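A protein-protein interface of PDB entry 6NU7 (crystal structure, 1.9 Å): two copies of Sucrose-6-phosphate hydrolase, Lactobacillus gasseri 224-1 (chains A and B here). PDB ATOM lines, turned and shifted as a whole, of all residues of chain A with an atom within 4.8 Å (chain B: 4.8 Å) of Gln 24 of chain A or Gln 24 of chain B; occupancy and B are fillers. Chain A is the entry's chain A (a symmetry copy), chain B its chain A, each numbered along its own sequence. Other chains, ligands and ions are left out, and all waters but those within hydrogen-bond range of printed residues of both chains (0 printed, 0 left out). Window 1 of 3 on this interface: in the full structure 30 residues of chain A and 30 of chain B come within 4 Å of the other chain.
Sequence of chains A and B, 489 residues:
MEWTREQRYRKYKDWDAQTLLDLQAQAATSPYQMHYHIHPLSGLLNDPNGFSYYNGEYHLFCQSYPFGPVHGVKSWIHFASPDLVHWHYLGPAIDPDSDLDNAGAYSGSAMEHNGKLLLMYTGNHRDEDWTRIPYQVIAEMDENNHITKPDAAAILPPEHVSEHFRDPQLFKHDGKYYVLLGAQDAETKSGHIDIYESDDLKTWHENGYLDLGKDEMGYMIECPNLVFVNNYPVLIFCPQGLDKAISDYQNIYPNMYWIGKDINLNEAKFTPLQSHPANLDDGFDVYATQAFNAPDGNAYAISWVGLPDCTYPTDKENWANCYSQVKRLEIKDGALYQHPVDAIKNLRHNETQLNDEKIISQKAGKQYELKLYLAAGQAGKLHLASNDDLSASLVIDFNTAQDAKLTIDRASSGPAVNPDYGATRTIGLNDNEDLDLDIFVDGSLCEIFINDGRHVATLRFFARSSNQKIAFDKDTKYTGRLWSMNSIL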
ATOM      1  N   LEU A  20     -13.462  22.548 -14.341  1.00  0.00           N
ATOM      2  CA  LEU A  20     -14.445  23.626 -14.292  1.00  0.00           C
ATOM      3  C   LEU A  20     -13.896  24.873 -13.589  1.00  0.00           C
ATOM      4  O   LEU A  20     -14.126  25.994 -14.048  1.00  0.00           O
ATOM      5  CB  LEU A  20     -15.722  23.152 -13.601  1.00  0.00           C
ATOM      6  CG  LEU A  20     -16.841  24.195 -13.423  1.00  0.00           C
ATOM      7  CD1 LEU A  20     -17.239  24.860 -14.738  1.00  0.00           C
ATOM      8  CD2 LEU A  20     -18.058  23.518 -12.802  1.00  0.00           C
ATOM      9  N   LEU A  21     -13.206  24.708 -12.453  1.00  0.00           N
ATOM     10  CA  LEU A  21     -12.623  25.880 -11.800  1.00  0.00           C
ATOM     11  C   LEU A  21     -11.607  26.569 -12.720  1.00  0.00           C
ATOM     12  O   LEU A  21     -11.593  27.805 -12.829  1.00  0.00           O
ATOM     13  CB  LEU A  21     -11.988  25.480 -10.459  1.00  0.00           C
ATOM     14  CG  LEU A  21     -13.083  25.131  -9.428  1.00  0.00           C
ATOM     15  CD1 LEU A  21     -12.522  24.252  -8.317  1.00  0.00           C
ATOM     16  CD2 LEU A  21     -13.778  26.389  -8.859  1.00  0.00           C
ATOM     17  N   ASP A  22     -10.771  25.785 -13.415  1.00  0.00           N
ATOM     18  CA  ASP A  22      -9.816  26.379 -14.350  1.00  0.00           C
ATOM     19  C   ASP A  22     -10.548  27.188 -15.410  1.00  0.00           C
ATOM     20  O   ASP A  22     -10.123  28.293 -15.782  1.00  0.00           O
ATOM     21  CB  ASP A  22      -8.982  25.297 -15.045  1.00  0.00           C
ATOM     22  CG  ASP A  22      -8.074  24.535 -14.103  1.00  0.00           C
ATOM     23  OD1 ASP A  22      -7.783  25.008 -12.987  1.00  0.00           O
ATOM     24  OD2 ASP A  22      -7.645  23.441 -14.508  1.00  0.00           O
ATOM     25  N   LEU A  23     -11.656  26.642 -15.914  1.00  0.00           N
ATOM     26  CA  LEU A  23     -12.400  27.305 -16.981  1.00  0.00           C
ATOM     27  C   LEU A  23     -13.033  28.600 -16.496  1.00  0.00           C
ATOM     28  O   LEU A  23     -13.193  29.547 -17.287  1.00  0.00           O
ATOM     29  CB  LEU A  23     -13.479  26.363 -17.533  1.00  0.00           C
ATOM     30  CG  LEU A  23     -12.953  25.193 -18.409  1.00  0.00           C
ATOM     31  CD1 LEU A  23     -14.054  24.154 -18.644  1.00  0.00           C
ATOM     32  CD2 LEU A  23     -12.425  25.750 -19.766  1.00  0.00           C
ATOM     33  N   GLN A  24     -13.457  28.641 -15.229  1.00  0.00           N
ATOM     34  CA  GLN A  24     -14.026  29.886 -14.705  1.00  0.00           C
ATOM     35  C   GLN A  24     -12.965  30.964 -14.656  1.00  0.00           C
ATOM     36  O   GLN A  24     -13.252  32.127 -14.962  1.00  0.00           O
ATOM     37  CB  GLN A  24     -14.618  29.687 -13.310  1.00  0.00           C
ATOM     38  CG  GLN A  24     -15.919  28.876 -13.354  1.00  0.00           C
ATOM     39  CD  GLN A  24     -16.591  28.721 -12.000  1.00  0.00           C
ATOM     40  OE1 GLN A  24     -15.944  28.815 -10.931  1.00  0.00           O
ATOM     41  NE2 GLN A  24     -17.902  28.449 -12.033  1.00  0.00           N
ATOM     42  N   ALA A  25     -11.739  30.596 -14.257  1.00  0.00           N
ATOM     43  CA  ALA A  25     -10.657  31.578 -14.231  1.00  0.00           C
ATOM     44  C   ALA A  25     -10.330  32.048 -15.642  1.00  0.00           C
ATOM     45  O   ALA A  25     -10.151  33.244 -15.884  1.00  0.00           O
ATOM     46  CB  ALA A  25      -9.417  30.996 -13.555  1.00  0.00           C
ATOM     47  N   GLN A  26     -10.275  31.117 -16.591  1.00  0.00           N
ATOM     48  CA  GLN A  26      -9.946  31.474 -17.963  1.00  0.00           C
ATOM     49  C   GLN A  26     -10.987  32.410 -18.573  1.00  0.00           C
ATOM     50  O   GLN A  26     -10.631  33.375 -19.262  1.00  0.00           O
ATOM     51  CB  GLN A  26      -9.812  30.205 -18.797  1.00  0.00           C
ATOM     52  CG  GLN A  26      -9.221  30.466 -20.165  1.00  0.00           C
ATOM     53  CD  GLN A  26      -8.771  29.186 -20.838  1.00  0.00           C
ATOM     54  OE1 GLN A  26      -9.288  28.083 -20.544  1.00  0.00           O
ATOM     55  NE2 GLN A  26      -7.781  29.314 -21.739  1.00  0.00           N
ATOM     56  N   ALA A  27     -12.273  32.128 -18.366  1.00  0.00           N
ATOM     57  CA  ALA A  27     -13.291  33.025 -18.884  1.00  0.00           C
ATOM     58  C   ALA A  27     -13.226  34.381 -18.193  1.00  0.00           C
ATOM     59  O   ALA A  27     -13.245  35.422 -18.856  1.00  0.00           O
ATOM     60  CB  ALA A  27     -14.684  32.414 -18.726  1.00  0.00           C
ATOM     61  N   ALA A  28     -13.164  34.393 -16.860  1.00  0.00           N
ATOM     62  CA  ALA A  28     -13.296  35.673 -16.155  1.00  0.00           C
ATOM     63  C   ALA A  28     -12.110  36.605 -16.413  1.00  0.00           C
ATOM     64  O   ALA A  28     -12.295  37.829 -16.479  1.00  0.00           O
ATOM     65  CB  ALA A  28     -13.461  35.431 -14.654  1.00  0.00           C
ATOM     66  N   LEU A  41     -19.991  32.388 -16.790  1.00  0.00           N
ATOM     67  CA  LEU A  41     -18.953  32.124 -15.803  1.00  0.00           C
ATOM     68  C   LEU A  41     -17.897  31.178 -16.363  1.00  0.00           C
ATOM     69  O   LEU A  41     -16.724  31.292 -16.003  1.00  0.00           O
ATOM     70  CB  LEU A  41     -19.560  31.570 -14.515  1.00  0.00           C
ATOM     71  CG  LEU A  41     -19.881  32.709 -13.543  1.00  0.00           C
ATOM     72  CD1 LEU A  41     -21.125  33.487 -14.028  1.00  0.00           C
ATOM     73  CD2 LEU A  41     -20.072  32.197 -12.134  1.00  0.00           C
ATOM     74  N   SER A  42     -18.283  30.264 -17.250  1.00  0.00           N
ATOM     75  CA  SER A  42     -17.371  29.356 -17.946  1.00  0.00           C
ATOM     76  C   SER A  42     -18.063  28.814 -19.192  1.00  0.00           C
ATOM     77  O   SER A  42     -19.290  28.738 -19.250  1.00  0.00           O
ATOM     78  CB  SER A  42     -16.912  28.199 -17.037  1.00  0.00           C
ATOM     79  OG  SER A  42     -17.954  27.225 -16.906  1.00  0.00           O
ATOM     80  N   TYR A  89     -25.373  36.239  -9.702  1.00  0.00           N
ATOM     81  CA  TYR A  89     -25.471  34.842 -10.123  1.00  0.00           C
ATOM     82  C   TYR A  89     -26.172  33.995  -9.069  1.00  0.00           C
ATOM     83  O   TYR A  89     -25.785  34.019  -7.895  1.00  0.00           O
ATOM     84  CB  TYR A  89     -24.065  34.299 -10.357  1.00  0.00           C
ATOM     85  CG  TYR A  89     -23.927  32.871 -10.865  1.00  0.00           C
ATOM     86  CD1 TYR A  89     -24.516  32.469 -12.057  1.00  0.00           C
ATOM     87  CD2 TYR A  89     -23.133  31.958 -10.180  1.00  0.00           C
ATOM     88  CE1 TYR A  89     -24.328  31.176 -12.534  1.00  0.00           C
ATOM     89  CE2 TYR A  89     -22.930  30.677 -10.645  1.00  0.00           C
ATOM     90  CZ  TYR A  89     -23.524  30.294 -11.808  1.00  0.00           C
ATOM     91  OH  TYR A  89     -23.321  29.006 -12.238  1.00  0.00           O
ATOM     92  N   LEU A  90     -27.191  33.233  -9.490  1.00  0.00           N
ATOM     93  CA  LEU A  90     -27.877  32.307  -8.600  1.00  0.00           C
ATOM     94  C   LEU A  90     -27.598  30.848  -8.937  1.00  0.00           C
ATOM     95  O   LEU A  90     -28.219  29.970  -8.335  1.00  0.00           O
ATOM     96  CB  LEU A  90     -29.393  32.561  -8.618  1.00  0.00           C
ATOM     97  CG  LEU A  90     -29.757  33.935  -8.052  1.00  0.00           C
ATOM     98  CD1 LEU A  90     -31.237  34.214  -8.237  1.00  0.00           C
ATOM     99  CD2 LEU A  90     -29.399  34.041  -6.551  1.00  0.00           C
ATOM    100  N   GLY A  91     -26.674  30.573  -9.868  1.00  0.00           N
ATOM    101  CA  GLY A  91     -26.265  29.222 -10.180  1.00  0.00           C
ATOM    102  C   GLY A  91     -27.145  28.487 -11.186  1.00  0.00           C
ATOM    103  O   GLY A  91     -28.118  29.014 -11.739  1.00  0.00           O
ATOM    104  N   PRO A  92     -26.816  27.221 -11.409  1.00  0.00           N
ATOM    105  CA  PRO A  92     -27.607  26.394 -12.334  1.00  0.00           C
ATOM    106  C   PRO A  92     -29.038  26.229 -11.840  1.00  0.00           C
ATOM    107  O   PRO A  92     -29.293  26.101 -10.639  1.00  0.00           O
ATOM    108  CB  PRO A  92     -26.857  25.049 -12.339  1.00  0.00           C
ATOM    109  CG  PRO A  92     -25.458  25.385 -11.839  1.00  0.00           C
ATOM    110  CD  PRO A  92     -25.675  26.494 -10.825  1.00  0.00           C
ATOM    111  N   LEU B  20     -19.956  20.291  -8.116  1.00  0.00           N
ATOM    112  CA  LEU B  20     -19.619  21.700  -7.937  1.00  0.00           C
ATOM    113  C   LEU B  20     -20.732  22.626  -8.441  1.00  0.00           C
ATOM    114  O   LEU B  20     -21.051  23.622  -7.787  1.00  0.00           O
ATOM    115  CB  LEU B  20     -18.304  22.027  -8.641  1.00  0.00           C
ATOM    116  CG  LEU B  20     -17.836  23.493  -8.589  1.00  0.00           C
ATOM    117  CD1 LEU B  20     -17.751  24.033  -7.164  1.00  0.00           C
ATOM    118  CD2 LEU B  20     -16.472  23.605  -9.262  1.00  0.00           C
ATOM    119  N   LEU B  21     -21.306  22.344  -9.618  1.00  0.00           N
ATOM    120  CA  LEU B  21     -22.411  23.181 -10.086  1.00  0.00           C
ATOM    121  C   LEU B  21     -23.591  23.126  -9.109  1.00  0.00           C
ATOM    122  O   LEU B  21     -24.195  24.162  -8.791  1.00  0.00           O
ATOM    123  CB  LEU B  21     -22.833  22.759 -11.502  1.00  0.00           C
ATOM    124  CG  LEU B  21     -21.752  23.164 -12.528  1.00  0.00           C
ATOM    125  CD1 LEU B  21     -21.867  22.327 -13.797  1.00  0.00           C
ATOM    126  CD2 LEU B  21     -21.776  24.677 -12.843  1.00  0.00           C
ATOM    127  N   ASP B  22     -23.913  21.930  -8.594  1.00  0.00           N
ATOM    128  CA  ASP B  22     -24.994  21.820  -7.615  1.00  0.00           C
ATOM    129  C   ASP B  22     -24.698  22.688  -6.401  1.00  0.00           C
ATOM    130  O   ASP B  22     -25.586  23.369  -5.866  1.00  0.00           O
ATOM    131  CB  ASP B  22     -25.170  20.370  -7.152  1.00  0.00           C
ATOM    132  CG  ASP B  22     -25.638  19.437  -8.250  1.00  0.00           C
ATOM    133  OD1 ASP B  22     -26.171  19.893  -9.280  1.00  0.00           O
ATOM    134  OD2 ASP B  22     -25.468  18.221  -8.056  1.00  0.00           O
ATOM    135  N   LEU B  23     -23.442  22.668  -5.950  1.00  0.00           N
ATOM    136  CA  LEU B  23     -23.064  23.414  -4.753  1.00  0.00           C
ATOM    137  C   LEU B  23     -23.157  24.915  -4.982  1.00  0.00           C
ATOM    138  O   LEU B  23     -23.439  25.671  -4.035  1.00  0.00           O
ATOM    139  CB  LEU B  23     -21.641  23.032  -4.323  1.00  0.00           C
ATOM    140  CG  LEU B  23     -21.497  21.624  -3.683  1.00  0.00           C
ATOM    141  CD1 LEU B  23     -20.023  21.223  -3.580  1.00  0.00           C
ATOM    142  CD2 LEU B  23     -22.169  21.616  -2.275  1.00  0.00           C
ATOM    143  N   GLN B  24     -22.863  25.371  -6.204  1.00  0.00           N
ATOM    144  CA  GLN B  24     -22.989  26.805  -6.481  1.00  0.00           C
ATOM    145  C   GLN B  24     -24.439  27.227  -6.393  1.00  0.00           C
ATOM    146  O   GLN B  24     -24.737  28.312  -5.881  1.00  0.00           O
ATOM    147  CB  GLN B  24     -22.437  27.158  -7.862  1.00  0.00           C
ATOM    148  CG  GLN B  24     -20.906  27.082  -7.900  1.00  0.00           C
ATOM    149  CD  GLN B  24     -20.303  27.503  -9.230  1.00  0.00           C
ATOM    150  OE1 GLN B  24     -20.962  27.453 -10.294  1.00  0.00           O
ATOM    151  NE2 GLN B  24     -19.023  27.897  -9.185  1.00  0.00           N
ATOM    152  N   ALA B  25     -25.352  26.386  -6.903  1.00  0.00           N
ATOM    153  CA  ALA B  25     -26.774  26.713  -6.809  1.00  0.00           C
ATOM    154  C   ALA B  25     -27.224  26.718  -5.354  1.00  0.00           C
ATOM    155  O   ALA B  25     -27.947  27.618  -4.920  1.00  0.00           O
ATOM    156  CB  ALA B  25     -27.607  25.729  -7.629  1.00  0.00           C
ATOM    157  N   GLN B  26     -26.781  25.730  -4.581  1.00  0.00           N
ATOM    158  CA  GLN B  26     -27.180  25.643  -3.185  1.00  0.00           C
ATOM    159  C   GLN B  26     -26.695  26.847  -2.378  1.00  0.00           C
ATOM    160  O   GLN B  26     -27.441  27.386  -1.551  1.00  0.00           O
ATOM    161  CB  GLN B  26     -26.648  24.347  -2.586  1.00  0.00           C
ATOM    162  CG  GLN B  26     -27.230  24.053  -1.221  1.00  0.00           C
ATOM    163  CD  GLN B  26     -26.975  22.621  -0.796  1.00  0.00           C
ATOM    164  OE1 GLN B  26     -26.004  21.973  -1.251  1.00  0.00           O
ATOM    165  NE2 GLN B  26     -27.864  22.099   0.069  1.00  0.00           N
ATOM    166  N   ALA B  27     -25.443  27.260  -2.574  1.00  0.00           N
ATOM    167  CA  ALA B  27     -24.962  28.434  -1.866  1.00  0.00           C
ATOM    168  C   ALA B  27     -25.704  29.685  -2.318  1.00  0.00           C
ATOM    169  O   ALA B  27     -26.161  30.476  -1.487  1.00  0.00           O
ATOM    170  CB  ALA B  27     -23.456  28.608  -2.063  1.00  0.00           C
ATOM    171  N   ALA B  28     -25.823  29.893  -3.631  1.00  0.00           N
ATOM    172  CA  ALA B  28     -26.357  31.176  -4.101  1.00  0.00           C
ATOM    173  C   ALA B  28     -27.832  31.360  -3.740  1.00  0.00           C
ATOM    174  O   ALA B  28     -28.259  32.490  -3.458  1.00  0.00           O
ATOM    175  CB  ALA B  28     -26.162  31.304  -5.612  1.00  0.00           C
ATOM    176  N   LEU B  41     -18.887  31.478  -3.739  1.00  0.00           N
ATOM    177  CA  LEU B  41     -19.711  30.918  -4.802  1.00  0.00           C
ATOM    178  C   LEU B  41     -20.153  29.500  -4.458  1.00  0.00           C
ATOM    179  O   LEU B  41     -21.250  29.093  -4.845  1.00  0.00           O
ATOM    180  CB  LEU B  41     -18.970  30.955  -6.137  1.00  0.00           C
ATOM    181  CG  LEU B  41     -19.283  32.254  -6.885  1.00  0.00           C
ATOM    182  CD1 LEU B  41     -18.548  33.440  -6.220  1.00  0.00           C
ATOM    183  CD2 LEU B  41     -18.930  32.147  -8.351  1.00  0.00           C
ATOM    184  N   SER B  42     -19.335  28.750  -3.723  1.00  0.00           N
ATOM    185  CA  SER B  42     -19.664  27.412  -3.234  1.00  0.00           C
ATOM    186  C   SER B  42     -18.742  27.067  -2.069  1.00  0.00           C
ATOM    187  O   SER B  42     -17.629  27.585  -1.970  1.00  0.00           O
ATOM    188  CB  SER B  42     -19.547  26.351  -4.346  1.00  0.00           C
ATOM    189  OG  SER B  42     -18.172  26.039  -4.595  1.00  0.00           O
ATOM    190  N   TYR B  89     -16.353  38.592  -9.822  1.00  0.00           N
ATOM    191  CA  TYR B  89     -15.574  37.367  -9.641  1.00  0.00           C
ATOM    192  C   TYR B  89     -14.599  37.158 -10.792  1.00  0.00           C
ATOM    193  O   TYR B  89     -15.000  37.193 -11.961  1.00  0.00           O
ATOM    194  CB  TYR B  89     -16.531  36.183  -9.565  1.00  0.00           C
ATOM    195  CG  TYR B  89     -15.940  34.803  -9.315  1.00  0.00           C
ATOM    196  CD1 TYR B  89     -15.178  34.539  -8.184  1.00  0.00           C
ATOM    197  CD2 TYR B  89     -16.224  33.752 -10.180  1.00  0.00           C
ATOM    198  CE1 TYR B  89     -14.698  33.256  -7.943  1.00  0.00           C
ATOM    199  CE2 TYR B  89     -15.763  32.475  -9.949  1.00  0.00           C
ATOM    200  CZ  TYR B  89     -15.007  32.234  -8.844  1.00  0.00           C
ATOM    201  OH  TYR B  89     -14.544  30.956  -8.649  1.00  0.00           O
ATOM    202  N   LEU B  90     -13.321  36.924 -10.462  1.00  0.00           N
ATOM    203  CA  LEU B  90     -12.313  36.611 -11.465  1.00  0.00           C
ATOM    204  C   LEU B  90     -11.838  35.166 -11.395  1.00  0.00           C
ATOM    205  O   LEU B  90     -10.898  34.814 -12.110  1.00  0.00           O
ATOM    206  CB  LEU B  90     -11.109  37.558 -11.337  1.00  0.00           C
ATOM    207  CG  LEU B  90     -11.479  39.011 -11.644  1.00  0.00           C
ATOM    208  CD1 LEU B  90     -10.311  39.933 -11.349  1.00  0.00           C
ATOM    209  CD2 LEU B  90     -11.909  39.185 -13.120  1.00  0.00           C
ATOM    210  N   GLY B  91     -12.472  34.325 -10.566  1.00  0.00           N
ATOM    211  CA  GLY B  91     -12.164  32.914 -10.508  1.00  0.00           C
ATOM    212  C   GLY B  91     -10.995  32.536  -9.603  1.00  0.00           C
ATOM    213  O   GLY B  91     -10.374  33.363  -8.926  1.00  0.00           O
ATOM    214  N   PRO B  92     -10.662  31.251  -9.614  1.00  0.00           N
ATOM    215  CA  PRO B  92      -9.530  30.765  -8.810  1.00  0.00           C
ATOM    216  C   PRO B  92      -8.221  31.399  -9.261  1.00  0.00           C
ATOM    217  O   PRO B  92      -7.988  31.616 -10.454  1.00  0.00           O
ATOM    218  CB  PRO B  92      -9.536  29.247  -9.067  1.00  0.00           C
ATOM    219  CG  PRO B  92     -10.944  28.945  -9.564  1.00  0.00           C
ATOM    220  CD  PRO B  92     -11.334  30.176 -10.364  1.00  0.00           C
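The side-chain amide nitrogen (NE2) of Gln 24 of chain B lies close to the side-chain amide nitrogen (NE2) of Gln 24 of chain A (3.1 Å). The side-chain amide oxygen (OE1) of Gln 24 of chain B sits at hydrogen-bond distance from the side-chain hydroxyl (OH) of Tyr 89 of chain A. The side-chain hydroxyl (OH) of Tyr 89 of chain B is in hydrogen-bond range of the side-chain amide oxygen (OE1) of Gln 24 of chain A (3.4 Å).
Leu 20 of chain B touches Leu 20 of chain A. Leu 21 of chain B touches Leu 20 of chain A (CG to CD2, 3.7 Å). Leu 21 of chain A touches Leu 20 of chain B (CG to CD2, 3.7 Å). Pro 92 of chain B touches Leu 21 of chain A. Ala 25 of chain A touches Leu 90 of chain B. CB of Ala 25 of chain A touches O of Pro 92 of chain B (3.5 Å). Ala 28 of chain A touches Tyr 89 of chain B. Leu 90 of chain B touches Ala 28 of chain A (CA to CB, 3.6 Å). Pro 92 of chain A touches Leu 21 of chain B (CD to O, 3.4 Å). Pro 92 of chain A touches Ala 25 of chain B.
Gln 24 of chain A touches just these residues of chain B: Gln 24 and Tyr 89. Printed residues of chain A within 4 Å of Gln 24 of chain B: Gln 24 (3.1 Å) and Tyr 89 (3.4 Å). Of the printed residues of chain B, Tyr 89 of chain A touches Gln 24 (3.4 Å) and Ala 28 (3.6 Å). Of the printed residues of chain A, Tyr 89 of chain B touches Gln 24 (3.4 Å) and Ala 28 (3.6 Å). The nearest residue of chain B that does not touch Gln 24 of chain A is Pro 92 of chain B (4.4 Å). The nearest printed residue of chain A that does not touch Leu 20 of chain B is Gln 24 of chain A (5.5 Å).
Hydrophobic or aromatic side chains of chain B within 4 Å of the printed part of chain A: Leu 20, Leu 21, Ala 25, Ala 28, Leu 41, Tyr 89, Leu 90 and Pro 92. Among the printed residues, 17 pairs touch across the chains. Among the printed residues, no Asp or Glu carboxylate lies within 4 Å of a Lys or Arg side-chain nitrogen of the other chain.
Leu 20 of chain A touches its own counterpart, Leu 20 of chain B. Ala 25 of chain A touches Leu 90 of chain B, and with the chains exchanged Leu 90 of chain A touches Ala 25 of chain B. Ala 28 of chain A touches Tyr 89 of chain B, and with the chains exchanged Tyr 89 of chain A touches Ala 28 of chain B. Leu 41 of chain A touches its own counterpart, Leu 41 of chain B. Of the 17 pairs that touch across the chains among the printed residues, 17 have their exchanged pair printed and touching as well.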
